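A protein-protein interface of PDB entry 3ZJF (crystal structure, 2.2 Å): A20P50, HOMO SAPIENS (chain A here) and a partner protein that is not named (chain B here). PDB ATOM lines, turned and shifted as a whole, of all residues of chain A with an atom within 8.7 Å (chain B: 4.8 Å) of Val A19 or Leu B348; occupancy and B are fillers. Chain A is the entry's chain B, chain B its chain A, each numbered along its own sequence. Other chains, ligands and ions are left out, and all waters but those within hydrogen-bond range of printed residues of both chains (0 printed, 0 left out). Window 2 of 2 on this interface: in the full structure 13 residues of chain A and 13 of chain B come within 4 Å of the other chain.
Of the 11 printed residues of chain B, 6 touch a printed residue of chain A.
Hydrophobic or aromatic side chains of chain B within 4 Å of the printed part of chain A: Pro B7, Leu B348 and His B351.
Along chain B the printed residues that touch a printed residue of chain A span positions 7 to 351.
Of the 20 printed residues of chain A, 5 touch a printed residue of chain B.
Among the printed residues, Asp or Glu carboxylates within 4 Å of a Lys or Arg side-chain nitrogen of the other chain: Arg A16 with Glu B347 (2.7 Å).
OH of Tyr B345 sits at hydrogen-bond distance from O of Pro B7, at 3.0 Å.
The backbone NH of Arg A16 sits close to the side-chain amide oxygen of Asn A14, at 3.5 Å.
NH1 of Arg A16 lies within salt-bridge range of OE2 of Glu A23 (3.8 Å).
The backbone carbonyl oxygen (O) of Arg A22 lies within hydrogen-bond range of the side-chain hydroxyl (OG1) of Thr A25, at 2.8 Å.
The side-chain hydroxyl (OG1) of Thr A118 is in hydrogen-bond range of the guanidinium group (NE) of Arg A22 (2.9 Å).
The guanidinium group of Arg A22 is in salt-bridge range of the side-chain carboxylate of Asp A119.
The backbone carbonyl oxygen (O) of Ser B13 sits at hydrogen-bond distance from the backbone NH (N) of Arg A16.
OE1 of Glu B347 lies within salt-bridge range of NE of Arg A16 (2.7 Å).
A ring nitrogen (NE2) of His B351 is in hydrogen-bond range of the side-chain carboxylate (OD2) of Asp A119, 3.4 Å away.
Among the printed residues, pairs that only touch across the chains: Val A19 with Leu B348, Met A15 with Ser B13, Arg A16 with Asp B344, Arg A22 with His B351, Met A15 with Pro B7, Met A15 with Leu B348 and Val A19 with His B351.
Printed residues of chain B within 4 Å of Arg A16: Ser B13 (3.2 Å), Asp B344 (3.6 Å) and Glu B347 (2.7 Å).
Printed residues of chain A within 4 Å of Ser B13: Met A15 (3.6 Å) and Arg A16 (3.2 Å).
Of the printed residues of chain A, Asp B344 touches Arg A16.
Of chain A, only Met A15 (3.7 Å) and Val A19 (3.5 Å) come within 4 Å of Leu B348.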
ATOM      1  N   TYR A  11     -26.243 -24.806  -7.415  1.00  0.00           N
ATOM      2  CA  TYR A  11     -25.044 -25.184  -8.186  1.00  0.00           C
ATOM      3  C   TYR A  11     -23.831 -24.262  -7.902  1.00  0.00           C
ATOM      4  O   TYR A  11     -22.693 -24.624  -8.185  1.00  0.00           O
ATOM      5  CB  TYR A  11     -25.340 -25.259  -9.710  1.00  0.00           C
ATOM      6  CG  TYR A  11     -25.286 -23.918 -10.433  1.00  0.00           C
ATOM      7  CD1 TYR A  11     -26.375 -23.051 -10.409  1.00  0.00           C
ATOM      8  CD2 TYR A  11     -24.134 -23.507 -11.121  1.00  0.00           C
ATOM      9  CE1 TYR A  11     -26.335 -21.820 -11.046  1.00  0.00           C
ATOM     10  CE2 TYR A  11     -24.083 -22.273 -11.768  1.00  0.00           C
ATOM     11  CZ  TYR A  11     -25.189 -21.430 -11.724  1.00  0.00           C
ATOM     12  OH  TYR A  11     -25.179 -20.199 -12.350  1.00  0.00           O
ATOM     13  N   ASN A  14     -20.685 -25.352  -5.359  1.00  0.00           N
ATOM     14  CA  ASN A  14     -19.485 -26.049  -5.786  1.00  0.00           C
ATOM     15  C   ASN A  14     -19.611 -26.351  -7.266  1.00  0.00           C
ATOM     16  O   ASN A  14     -20.000 -27.468  -7.628  1.00  0.00           O
ATOM     17  CB  ASN A  14     -19.235 -27.336  -4.965  1.00  0.00           C
ATOM     18  CG  ASN A  14     -17.810 -27.901  -5.139  1.00  0.00           C
ATOM     19  OD1 ASN A  14     -17.124 -27.627  -6.131  1.00  0.00           O
ATOM     20  ND2 ASN A  14     -17.386 -28.723  -4.186  1.00  0.00           N
ATOM     21  N   MET A  15     -19.243 -25.377  -8.111  1.00  0.00           N
ATOM     22  CA  MET A  15     -19.484 -25.492  -9.544  1.00  0.00           C
ATOM     23  C   MET A  15     -18.686 -26.641 -10.112  1.00  0.00           C
ATOM     24  O   MET A  15     -19.110 -27.286 -11.065  1.00  0.00           O
ATOM     25  CB  MET A  15     -19.175 -24.191 -10.299  1.00  0.00           C
ATOM     26  CG  MET A  15     -20.077 -23.017  -9.995  1.00  0.00           C
ATOM     27  SD  MET A  15     -19.790 -21.724 -11.219  1.00  0.00           S
ATOM     28  CE  MET A  15     -20.316 -22.564 -12.714  1.00  0.00           C
ATOM     29  N   ARG A  16     -17.526 -26.897  -9.507  1.00  0.00           N
ATOM     30  CA  ARG A  16     -16.632 -27.955  -9.987  1.00  0.00           C
ATOM     31  C   ARG A  16     -17.194 -29.342  -9.664  1.00  0.00           C
ATOM     32  O   ARG A  16     -17.134 -30.234 -10.491  1.00  0.00           O
ATOM     33  CB  ARG A  16     -15.229 -27.819  -9.411  1.00  0.00           C
ATOM     34  CG  ARG A  16     -14.272 -28.944  -9.830  1.00  0.00           C
ATOM     35  CD  ARG A  16     -14.178 -29.031 -11.352  1.00  0.00           C
ATOM     36  NE  ARG A  16     -13.321 -30.113 -11.853  1.00  0.00           N
ATOM     37  CZ  ARG A  16     -13.732 -31.342 -12.185  1.00  0.00           C
ATOM     38  NH1 ARG A  16     -15.011 -31.709 -12.055  1.00  0.00           N
ATOM     39  NH2 ARG A  16     -12.849 -32.223 -12.650  1.00  0.00           N
ATOM     40  N   LYS A  17     -17.677 -29.527  -8.449  1.00  0.00           N
ATOM     41  CA  LYS A  17     -18.291 -30.798  -8.079  1.00  0.00           C
ATOM     42  C   LYS A  17     -19.511 -31.081  -8.994  1.00  0.00           C
ATOM     43  O   LYS A  17     -19.676 -32.191  -9.476  1.00  0.00           O
ATOM     44  CB  LYS A  17     -18.614 -30.829  -6.576  1.00  0.00           C
ATOM     45  CG  LYS A  17     -19.472 -32.020  -6.104  1.00  0.00           C
ATOM     46  CD  LYS A  17     -19.692 -31.989  -4.572  1.00  0.00           C
ATOM     47  CE  LYS A  17     -18.418 -32.265  -3.762  1.00  0.00           C
ATOM     48  NZ  LYS A  17     -18.677 -32.071  -2.299  1.00  0.00           N
ATOM     49  N   ALA A  18     -20.295 -30.052  -9.305  1.00  0.00           N
ATOM     50  CA  ALA A  18     -21.456 -30.218 -10.185  1.00  0.00           C
ATOM     51  C   ALA A  18     -21.087 -30.759 -11.561  1.00  0.00           C
ATOM     52  O   ALA A  18     -21.756 -31.662 -12.083  1.00  0.00           O
ATOM     53  CB  ALA A  18     -22.274 -28.914 -10.310  1.00  0.00           C
ATOM     54  N   VAL A  19     -20.025 -30.207 -12.144  1.00  0.00           N
ATOM     55  CA  VAL A  19     -19.494 -30.711 -13.391  1.00  0.00           C
ATOM     56  C   VAL A  19     -19.102 -32.186 -13.294  1.00  0.00           C
ATOM     57  O   VAL A  19     -19.392 -32.965 -14.198  1.00  0.00           O
ATOM     58  CB  VAL A  19     -18.240 -29.880 -13.860  1.00  0.00           C
ATOM     59  CG1 VAL A  19     -17.288 -30.762 -14.641  1.00  0.00           C
ATOM     60  CG2 VAL A  19     -18.679 -28.701 -14.680  1.00  0.00           C
ATOM     61  N   LYS A  20     -18.426 -32.568 -12.212  1.00  0.00           N
ATOM     62  CA  LYS A  20     -18.028 -33.960 -12.027  1.00  0.00           C
ATOM     63  C   LYS A  20     -19.260 -34.881 -11.915  1.00  0.00           C
ATOM     64  O   LYS A  20     -19.261 -35.992 -12.464  1.00  0.00           O
ATOM     65  CB  LYS A  20     -17.139 -34.114 -10.793  1.00  0.00           C
ATOM     66  CG  LYS A  20     -16.520 -35.500 -10.656  1.00  0.00           C
ATOM     67  CD  LYS A  20     -15.777 -35.670  -9.337  1.00  0.00           C
ATOM     68  CE  LYS A  20     -16.756 -35.718  -8.175  1.00  0.00           C
ATOM     69  NZ  LYS A  20     -16.069 -35.938  -6.874  1.00  0.00           N
ATOM     70  N   ILE A  21     -20.296 -34.415 -11.212  1.00  0.00           N
ATOM     71  CA  ILE A  21     -21.517 -35.209 -11.075  1.00  0.00           C
ATOM     72  C   ILE A  21     -22.097 -35.505 -12.446  1.00  0.00           C
ATOM     73  O   ILE A  21     -22.313 -36.664 -12.790  1.00  0.00           O
ATOM     74  CB  ILE A  21     -22.598 -34.527 -10.209  1.00  0.00           C
ATOM     75  CG1 ILE A  21     -22.088 -34.292  -8.786  1.00  0.00           C
ATOM     76  CG2 ILE A  21     -23.857 -35.409 -10.169  1.00  0.00           C
ATOM     77  CD1 ILE A  21     -22.983 -33.437  -7.929  1.00  0.00           C
ATOM     78  N   ARG A  22     -22.309 -34.457 -13.243  1.00  0.00           N
ATOM     79  CA  ARG A  22     -22.872 -34.628 -14.581  1.00  0.00           C
ATOM     80  C   ARG A  22     -21.974 -35.474 -15.482  1.00  0.00           C
ATOM     81  O   ARG A  22     -22.487 -36.225 -16.305  1.00  0.00           O
ATOM     82  CB  ARG A  22     -23.207 -33.286 -15.234  1.00  0.00           C
ATOM     83  CG  ARG A  22     -24.466 -32.628 -14.680  1.00  0.00           C
ATOM     84  CD  ARG A  22     -24.785 -31.318 -15.407  1.00  0.00           C
ATOM     85  NE  ARG A  22     -24.135 -30.158 -14.799  1.00  0.00           N
ATOM     86  CZ  ARG A  22     -23.055 -29.556 -15.287  1.00  0.00           C
ATOM     87  NH1 ARG A  22     -22.487 -29.989 -16.406  1.00  0.00           N
ATOM     88  NH2 ARG A  22     -22.539 -28.513 -14.654  1.00  0.00           N
ATOM     89  N   GLU A  23     -20.653 -35.371 -15.318  1.00  0.00           N
ATOM     90  CA  GLU A  23     -19.719 -36.236 -16.055  1.00  0.00           C
ATOM     91  C   GLU A  23     -19.931 -37.727 -15.780  1.00  0.00           C
ATOM     92  O   GLU A  23     -19.781 -38.546 -16.681  1.00  0.00           O
ATOM     93  CB  GLU A  23     -18.250 -35.894 -15.748  1.00  0.00           C
ATOM     94  CG  GLU A  23     -17.777 -34.559 -16.260  1.00  0.00           C
ATOM     95  CD  GLU A  23     -16.253 -34.398 -16.136  1.00  0.00           C
ATOM     96  OE1 GLU A  23     -15.548 -34.903 -17.028  1.00  0.00           O
ATOM     97  OE2 GLU A  23     -15.768 -33.801 -15.137  1.00  0.00           O
ATOM     98  N   ARG A  24     -20.231 -38.088 -14.535  1.00  0.00           N
ATOM     99  CA  ARG A  24     -20.490 -39.492 -14.215  1.00  0.00           C
ATOM    100  C   ARG A  24     -21.757 -40.053 -14.902  1.00  0.00           C
ATOM    101  O   ARG A  24     -21.806 -41.234 -15.257  1.00  0.00           O
ATOM    102  CB  ARG A  24     -20.573 -39.714 -12.700  1.00  0.00           C
ATOM    103  CG  ARG A  24     -19.229 -39.892 -12.026  1.00  0.00           C
ATOM    104  CD  ARG A  24     -19.395 -40.513 -10.643  1.00  0.00           C
ATOM    105  NE  ARG A  24     -18.214 -40.279  -9.813  1.00  0.00           N
ATOM    106  CZ  ARG A  24     -18.214 -40.336  -8.485  1.00  0.00           C
ATOM    107  NH1 ARG A  24     -19.336 -40.627  -7.837  1.00  0.00           N
ATOM    108  NH2 ARG A  24     -17.097 -40.101  -7.806  1.00  0.00           N
ATOM    109  N   THR A  25     -22.755 -39.195 -15.106  1.00  0.00           N
ATOM    110  CA  THR A  25     -24.076 -39.651 -15.558  1.00  0.00           C
ATOM    111  C   THR A  25     -24.125 -40.473 -16.869  1.00  0.00           C
ATOM    112  O   THR A  25     -24.716 -41.556 -16.870  1.00  0.00           O
ATOM    113  CB  THR A  25     -25.184 -38.545 -15.478  1.00  0.00           C
ATOM    114  OG1 THR A  25     -24.944 -37.497 -16.416  1.00  0.00           O
ATOM    115  CG2 THR A  25     -25.235 -37.959 -14.092  1.00  0.00           C
ATOM    116  N   PRO A  26     -23.481 -39.992 -17.962  1.00  0.00           N
ATOM    117  CA  PRO A  26     -23.550 -40.712 -19.242  1.00  0.00           C
ATOM    118  C   PRO A  26     -22.870 -42.076 -19.207  1.00  0.00           C
ATOM    119  O   PRO A  26     -23.313 -42.986 -19.902  1.00  0.00           O
ATOM    120  CB  PRO A  26     -22.774 -39.804 -20.207  1.00  0.00           C
ATOM    121  CG  PRO A  26     -22.718 -38.485 -19.559  1.00  0.00           C
ATOM    122  CD  PRO A  26     -22.707 -38.748 -18.089  1.00  0.00           C
ATOM    123  N   VAL A 115     -28.010 -31.993  -8.857  1.00  0.00           N
ATOM    124  CA  VAL A 115     -27.724 -31.139 -10.029  1.00  0.00           C
ATOM    125  C   VAL A 115     -28.851 -31.149 -11.062  1.00  0.00           C
ATOM    126  O   VAL A 115     -29.701 -32.056 -11.060  1.00  0.00           O
ATOM    127  CB  VAL A 115     -26.429 -31.542 -10.771  1.00  0.00           C
ATOM    128  CG1 VAL A 115     -25.194 -31.240  -9.913  1.00  0.00           C
ATOM    129  CG2 VAL A 115     -26.460 -32.994 -11.228  1.00  0.00           C
ATOM    130  N   GLN A 116     -28.856 -30.159 -11.956  1.00  0.00           N
ATOM    131  CA  GLN A 116     -29.903 -30.096 -12.981  1.00  0.00           C
ATOM    132  C   GLN A 116     -29.422 -30.782 -14.269  1.00  0.00           C
ATOM    133  O   GLN A 116     -28.285 -31.259 -14.323  1.00  0.00           O
ATOM    134  CB  GLN A 116     -30.462 -28.661 -13.158  1.00  0.00           C
ATOM    135  CG  GLN A 116     -31.272 -28.191 -11.908  1.00  0.00           C
ATOM    136  CD  GLN A 116     -31.930 -26.819 -12.007  1.00  0.00           C
ATOM    137  OE1 GLN A 116     -32.792 -26.581 -12.841  1.00  0.00           O
ATOM    138  NE2 GLN A 116     -31.531 -25.915 -11.121  1.00  0.00           N
ATOM    139  N   THR A 118     -28.389 -29.973 -17.065  1.00  0.00           N
ATOM    140  CA  THR A 118     -27.860 -28.914 -17.914  1.00  0.00           C
ATOM    141  C   THR A 118     -27.036 -29.432 -19.099  1.00  0.00           C
ATOM    142  O   THR A 118     -26.964 -28.778 -20.123  1.00  0.00           O
ATOM    143  CB  THR A 118     -27.050 -27.933 -17.087  1.00  0.00           C
ATOM    144  OG1 THR A 118     -26.165 -28.669 -16.240  1.00  0.00           O
ATOM    145  CG2 THR A 118     -27.972 -27.097 -16.210  1.00  0.00           C
ATOM    146  N   ASP A 119     -26.434 -30.611 -18.962  1.00  0.00           N
ATOM    147  CA  ASP A 119     -25.787 -31.274 -20.090  1.00  0.00           C
ATOM    148  C   ASP A 119     -26.741 -32.149 -20.891  1.00  0.00           C
ATOM    149  O   ASP A 119     -26.302 -32.880 -21.773  1.00  0.00           O
ATOM    150  CB  ASP A 119     -24.606 -32.120 -19.624  1.00  0.00           C
ATOM    151  CG  ASP A 119     -23.448 -31.278 -19.136  1.00  0.00           C
ATOM    152  OD1 ASP A 119     -23.463 -30.054 -19.386  1.00  0.00           O
ATOM    153  OD2 ASP A 119     -22.529 -31.838 -18.500  1.00  0.00           O
ATOM    154  N   ILE A 339     -20.341 -36.379  -4.096  1.00  0.00           N
ATOM    155  CA  ILE A 339     -21.240 -35.970  -5.171  1.00  0.00           C
ATOM    156  C   ILE A 339     -22.528 -35.320  -4.640  1.00  0.00           C
ATOM    157  O   ILE A 339     -23.637 -35.537  -5.183  1.00  0.00           O
ATOM    158  CB  ILE A 339     -21.544 -37.135  -6.143  1.00  0.00           C
ATOM    159  CG1 ILE A 339     -22.151 -38.315  -5.379  1.00  0.00           C
ATOM    160  CG2 ILE A 339     -20.293 -37.595  -6.858  1.00  0.00           C
ATOM    161  CD1 ILE A 339     -22.268 -39.573  -6.205  1.00  0.00           C
ATOM    162  N   LEU A 341     -24.021 -31.540  -3.799  1.00  0.00           N
ATOM    163  CA  LEU A 341     -23.964 -30.083  -3.694  1.00  0.00           C
ATOM    164  C   LEU A 341     -24.615 -29.572  -2.396  1.00  0.00           C
ATOM    165  O   LEU A 341     -24.169 -28.564  -1.802  1.00  0.00           O
ATOM    166  CB  LEU A 341     -24.569 -29.394  -4.931  1.00  0.00           C
ATOM    167  CG  LEU A 341     -23.913 -29.470  -6.316  1.00  0.00           C
ATOM    168  CD1 LEU A 341     -24.774 -28.728  -7.349  1.00  0.00           C
ATOM    169  CD2 LEU A 341     -22.482 -28.901  -6.330  1.00  0.00           C
ATOM    170  N   PRO B   7     -17.736 -19.539 -14.793  1.00  0.00           N
ATOM    171  CA  PRO B   7     -18.049 -18.592 -13.711  1.00  0.00           C
ATOM    172  C   PRO B   7     -17.478 -17.218 -13.998  1.00  0.00           C
ATOM    173  O   PRO B   7     -16.493 -17.099 -14.731  1.00  0.00           O
ATOM    174  CB  PRO B   7     -17.377 -19.207 -12.470  1.00  0.00           C
ATOM    175  CG  PRO B   7     -16.313 -20.103 -13.000  1.00  0.00           C
ATOM    176  CD  PRO B   7     -16.779 -20.580 -14.365  1.00  0.00           C
ATOM    177  N   SER B  13     -15.777 -20.746  -8.649  1.00  0.00           N
ATOM    178  CA  SER B  13     -15.558 -22.085  -9.188  1.00  0.00           C
ATOM    179  C   SER B  13     -15.633 -23.171  -8.118  1.00  0.00           C
ATOM    180  O   SER B  13     -15.851 -24.340  -8.437  1.00  0.00           O
ATOM    181  CB  SER B  13     -14.229 -22.178  -9.938  1.00  0.00           C
ATOM    182  OG  SER B  13     -13.147 -22.438  -9.041  1.00  0.00           O
ATOM    183  N   ASP B 344      -9.420 -25.688 -10.155  1.00  0.00           N
ATOM    184  CA  ASP B 344     -10.808 -26.076 -10.356  1.00  0.00           C
ATOM    185  C   ASP B 344     -11.329 -25.216 -11.470  1.00  0.00           C
ATOM    186  O   ASP B 344     -12.121 -25.686 -12.297  1.00  0.00           O
ATOM    187  CB  ASP B 344     -11.643 -25.897  -9.094  1.00  0.00           C
ATOM    188  CG  ASP B 344     -11.309 -26.900  -8.049  1.00  0.00           C
ATOM    189  OD1 ASP B 344     -11.107 -28.080  -8.384  1.00  0.00           O
ATOM    190  OD2 ASP B 344     -11.233 -26.502  -6.886  1.00  0.00           O
ATOM    191  N   TYR B 345     -10.831 -23.974 -11.524  1.00  0.00           N
ATOM    192  CA  TYR B 345     -11.301 -23.067 -12.558  1.00  0.00           C
ATOM    193  C   TYR B 345     -10.875 -23.615 -13.917  1.00  0.00           C
ATOM    194  O   TYR B 345     -11.682 -23.724 -14.848  1.00  0.00           O
ATOM    195  CB  TYR B 345     -10.814 -21.639 -12.352  1.00  0.00           C
ATOM    196  CG  TYR B 345     -11.568 -20.662 -13.228  1.00  0.00           C
ATOM    197  CD1 TYR B 345     -11.253 -20.506 -14.573  1.00  0.00           C
ATOM    198  CD2 TYR B 345     -12.612 -19.912 -12.715  1.00  0.00           C
ATOM    199  CE1 TYR B 345     -11.952 -19.626 -15.378  1.00  0.00           C
ATOM    200  CE2 TYR B 345     -13.320 -19.020 -13.523  1.00  0.00           C
ATOM    201  CZ  TYR B 345     -13.002 -18.895 -14.845  1.00  0.00           C
ATOM    202  OH  TYR B 345     -13.727 -18.021 -15.622  1.00  0.00           O
ATOM    203  N   PHE B 346      -9.616 -24.017 -13.999  1.00  0.00           N
ATOM    204  CA  PHE B 346      -9.074 -24.567 -15.229  1.00  0.00           C
ATOM    205  C   PHE B 346      -9.913 -25.735 -15.717  1.00  0.00           C
ATOM    206  O   PHE B 346     -10.217 -25.846 -16.905  1.00  0.00           O
ATOM    207  CB  PHE B 346      -7.627 -25.011 -15.005  1.00  0.00           C
ATOM    208  CG  PHE B 346      -6.933 -25.446 -16.251  1.00  0.00           C
ATOM    209  CD1 PHE B 346      -6.785 -24.574 -17.317  1.00  0.00           C
ATOM    210  CD2 PHE B 346      -6.418 -26.730 -16.358  1.00  0.00           C
ATOM    211  CE1 PHE B 346      -6.135 -24.976 -18.473  1.00  0.00           C
ATOM    212  CE2 PHE B 346      -5.775 -27.145 -17.512  1.00  0.00           C
ATOM    213  CZ  PHE B 346      -5.632 -26.268 -18.571  1.00  0.00           C
ATOM    214  N   GLU B 347     -10.288 -26.597 -14.788  1.00  0.00           N
ATOM    215  CA  GLU B 347     -11.049 -27.794 -15.108  1.00  0.00           C
ATOM    216  C   GLU B 347     -12.484 -27.522 -15.582  1.00  0.00           C
ATOM    217  O   GLU B 347     -13.007 -28.257 -16.416  1.00  0.00           O
ATOM    218  CB  GLU B 347     -11.037 -28.742 -13.917  1.00  0.00           C
ATOM    219  CG  GLU B 347      -9.726 -29.483 -13.759  1.00  0.00           C
ATOM    220  CD  GLU B 347      -9.658 -30.268 -12.467  1.00  0.00           C
ATOM    221  OE1 GLU B 347     -10.628 -30.209 -11.676  1.00  0.00           O
ATOM    222  OE2 GLU B 347      -8.630 -30.941 -12.240  1.00  0.00           O
ATOM    223  N   LEU B 348     -13.126 -26.489 -15.046  1.00  0.00           N
ATOM    224  CA  LEU B 348     -14.370 -26.007 -15.625  1.00  0.00           C
ATOM    225  C   LEU B 348     -14.175 -25.537 -17.066  1.00  0.00           C
ATOM    226  O   LEU B 348     -15.011 -25.805 -17.925  1.00  0.00           O
ATOM    227  CB  LEU B 348     -14.947 -24.877 -14.783  1.00  0.00           C
ATOM    228  CG  LEU B 348     -15.612 -25.258 -13.459  1.00  0.00           C
ATOM    229  CD1 LEU B 348     -15.736 -24.061 -12.561  1.00  0.00           C
ATOM    230  CD2 LEU B 348     -16.978 -25.820 -13.732  1.00  0.00           C
ATOM    231  N   VAL B 349     -13.056 -24.847 -17.320  1.00  0.00           N
ATOM    232  CA  VAL B 349     -12.733 -24.310 -18.638  1.00  0.00           C
ATOM    233  C   VAL B 349     -12.612 -25.425 -19.652  1.00  0.00           C
ATOM    234  O   VAL B 349     -13.227 -25.377 -20.716  1.00  0.00           O
ATOM    235  CB  VAL B 349     -11.410 -23.506 -18.626  1.00  0.00           C
ATOM    236  CG1 VAL B 349     -11.028 -23.116 -20.040  1.00  0.00           C
ATOM    237  CG2 VAL B 349     -11.547 -22.284 -17.754  1.00  0.00           C
ATOM    238  N   GLN B 350     -11.835 -26.446 -19.315  1.00  0.00           N
ATOM    239  CA  GLN B 350     -11.752 -27.638 -20.156  1.00  0.00           C
ATOM    240  C   GLN B 350     -13.121 -28.270 -20.482  1.00  0.00           C
ATOM    241  O   GLN B 350     -13.445 -28.466 -21.648  1.00  0.00           O
ATOM    242  CB  GLN B 350     -10.798 -28.659 -19.533  1.00  0.00           C
ATOM    243  CG  GLN B 350      -9.345 -28.166 -19.531  1.00  0.00           C
ATOM    244  CD  GLN B 350      -8.350 -29.249 -19.177  1.00  0.00           C
ATOM    245  OE1 GLN B 350      -7.343 -29.434 -19.867  1.00  0.00           O
ATOM    246  NE2 GLN B 350      -8.627 -29.976 -18.097  1.00  0.00           N
ATOM    247  N   HIS B 351     -13.911 -28.576 -19.453  1.00  0.00           N
ATOM    248  CA  HIS B 351     -15.245 -29.135 -19.642  1.00  0.00           C
ATOM    249  C   HIS B 351     -16.073 -28.308 -20.615  1.00  0.00           C
ATOM    250  O   HIS B 351     -16.614 -28.833 -21.586  1.00  0.00           O
ATOM    251  CB  HIS B 351     -15.983 -29.246 -18.308  1.00  0.00           C
ATOM    252  CG  HIS B 351     -17.370 -29.803 -18.429  1.00  0.00           C
ATOM    253  ND1 HIS B 351     -17.626 -31.155 -18.528  1.00  0.00           N
ATOM    254  CD2 HIS B 351     -18.575 -29.190 -18.467  1.00  0.00           C
ATOM    255  CE1 HIS B 351     -18.927 -31.351 -18.626  1.00  0.00           C
ATOM    256  NE2 HIS B 351     -19.527 -30.175 -18.596  1.00  0.00           N
ATOM    257  N   GLU B 352     -16.154 -27.009 -20.364  1.00  0.00           N
ATOM    258  CA  GLU B 352     -16.955 -26.137 -21.202  1.00  0.00           C
ATOM    259  C   GLU B 352     -16.391 -25.956 -22.620  1.00  0.00           C
ATOM    260  O   GLU B 352     -17.104 -25.523 -23.521  1.00  0.00           O
ATOM    261  CB  GLU B 352     -17.144 -24.788 -20.517  1.00  0.00           C
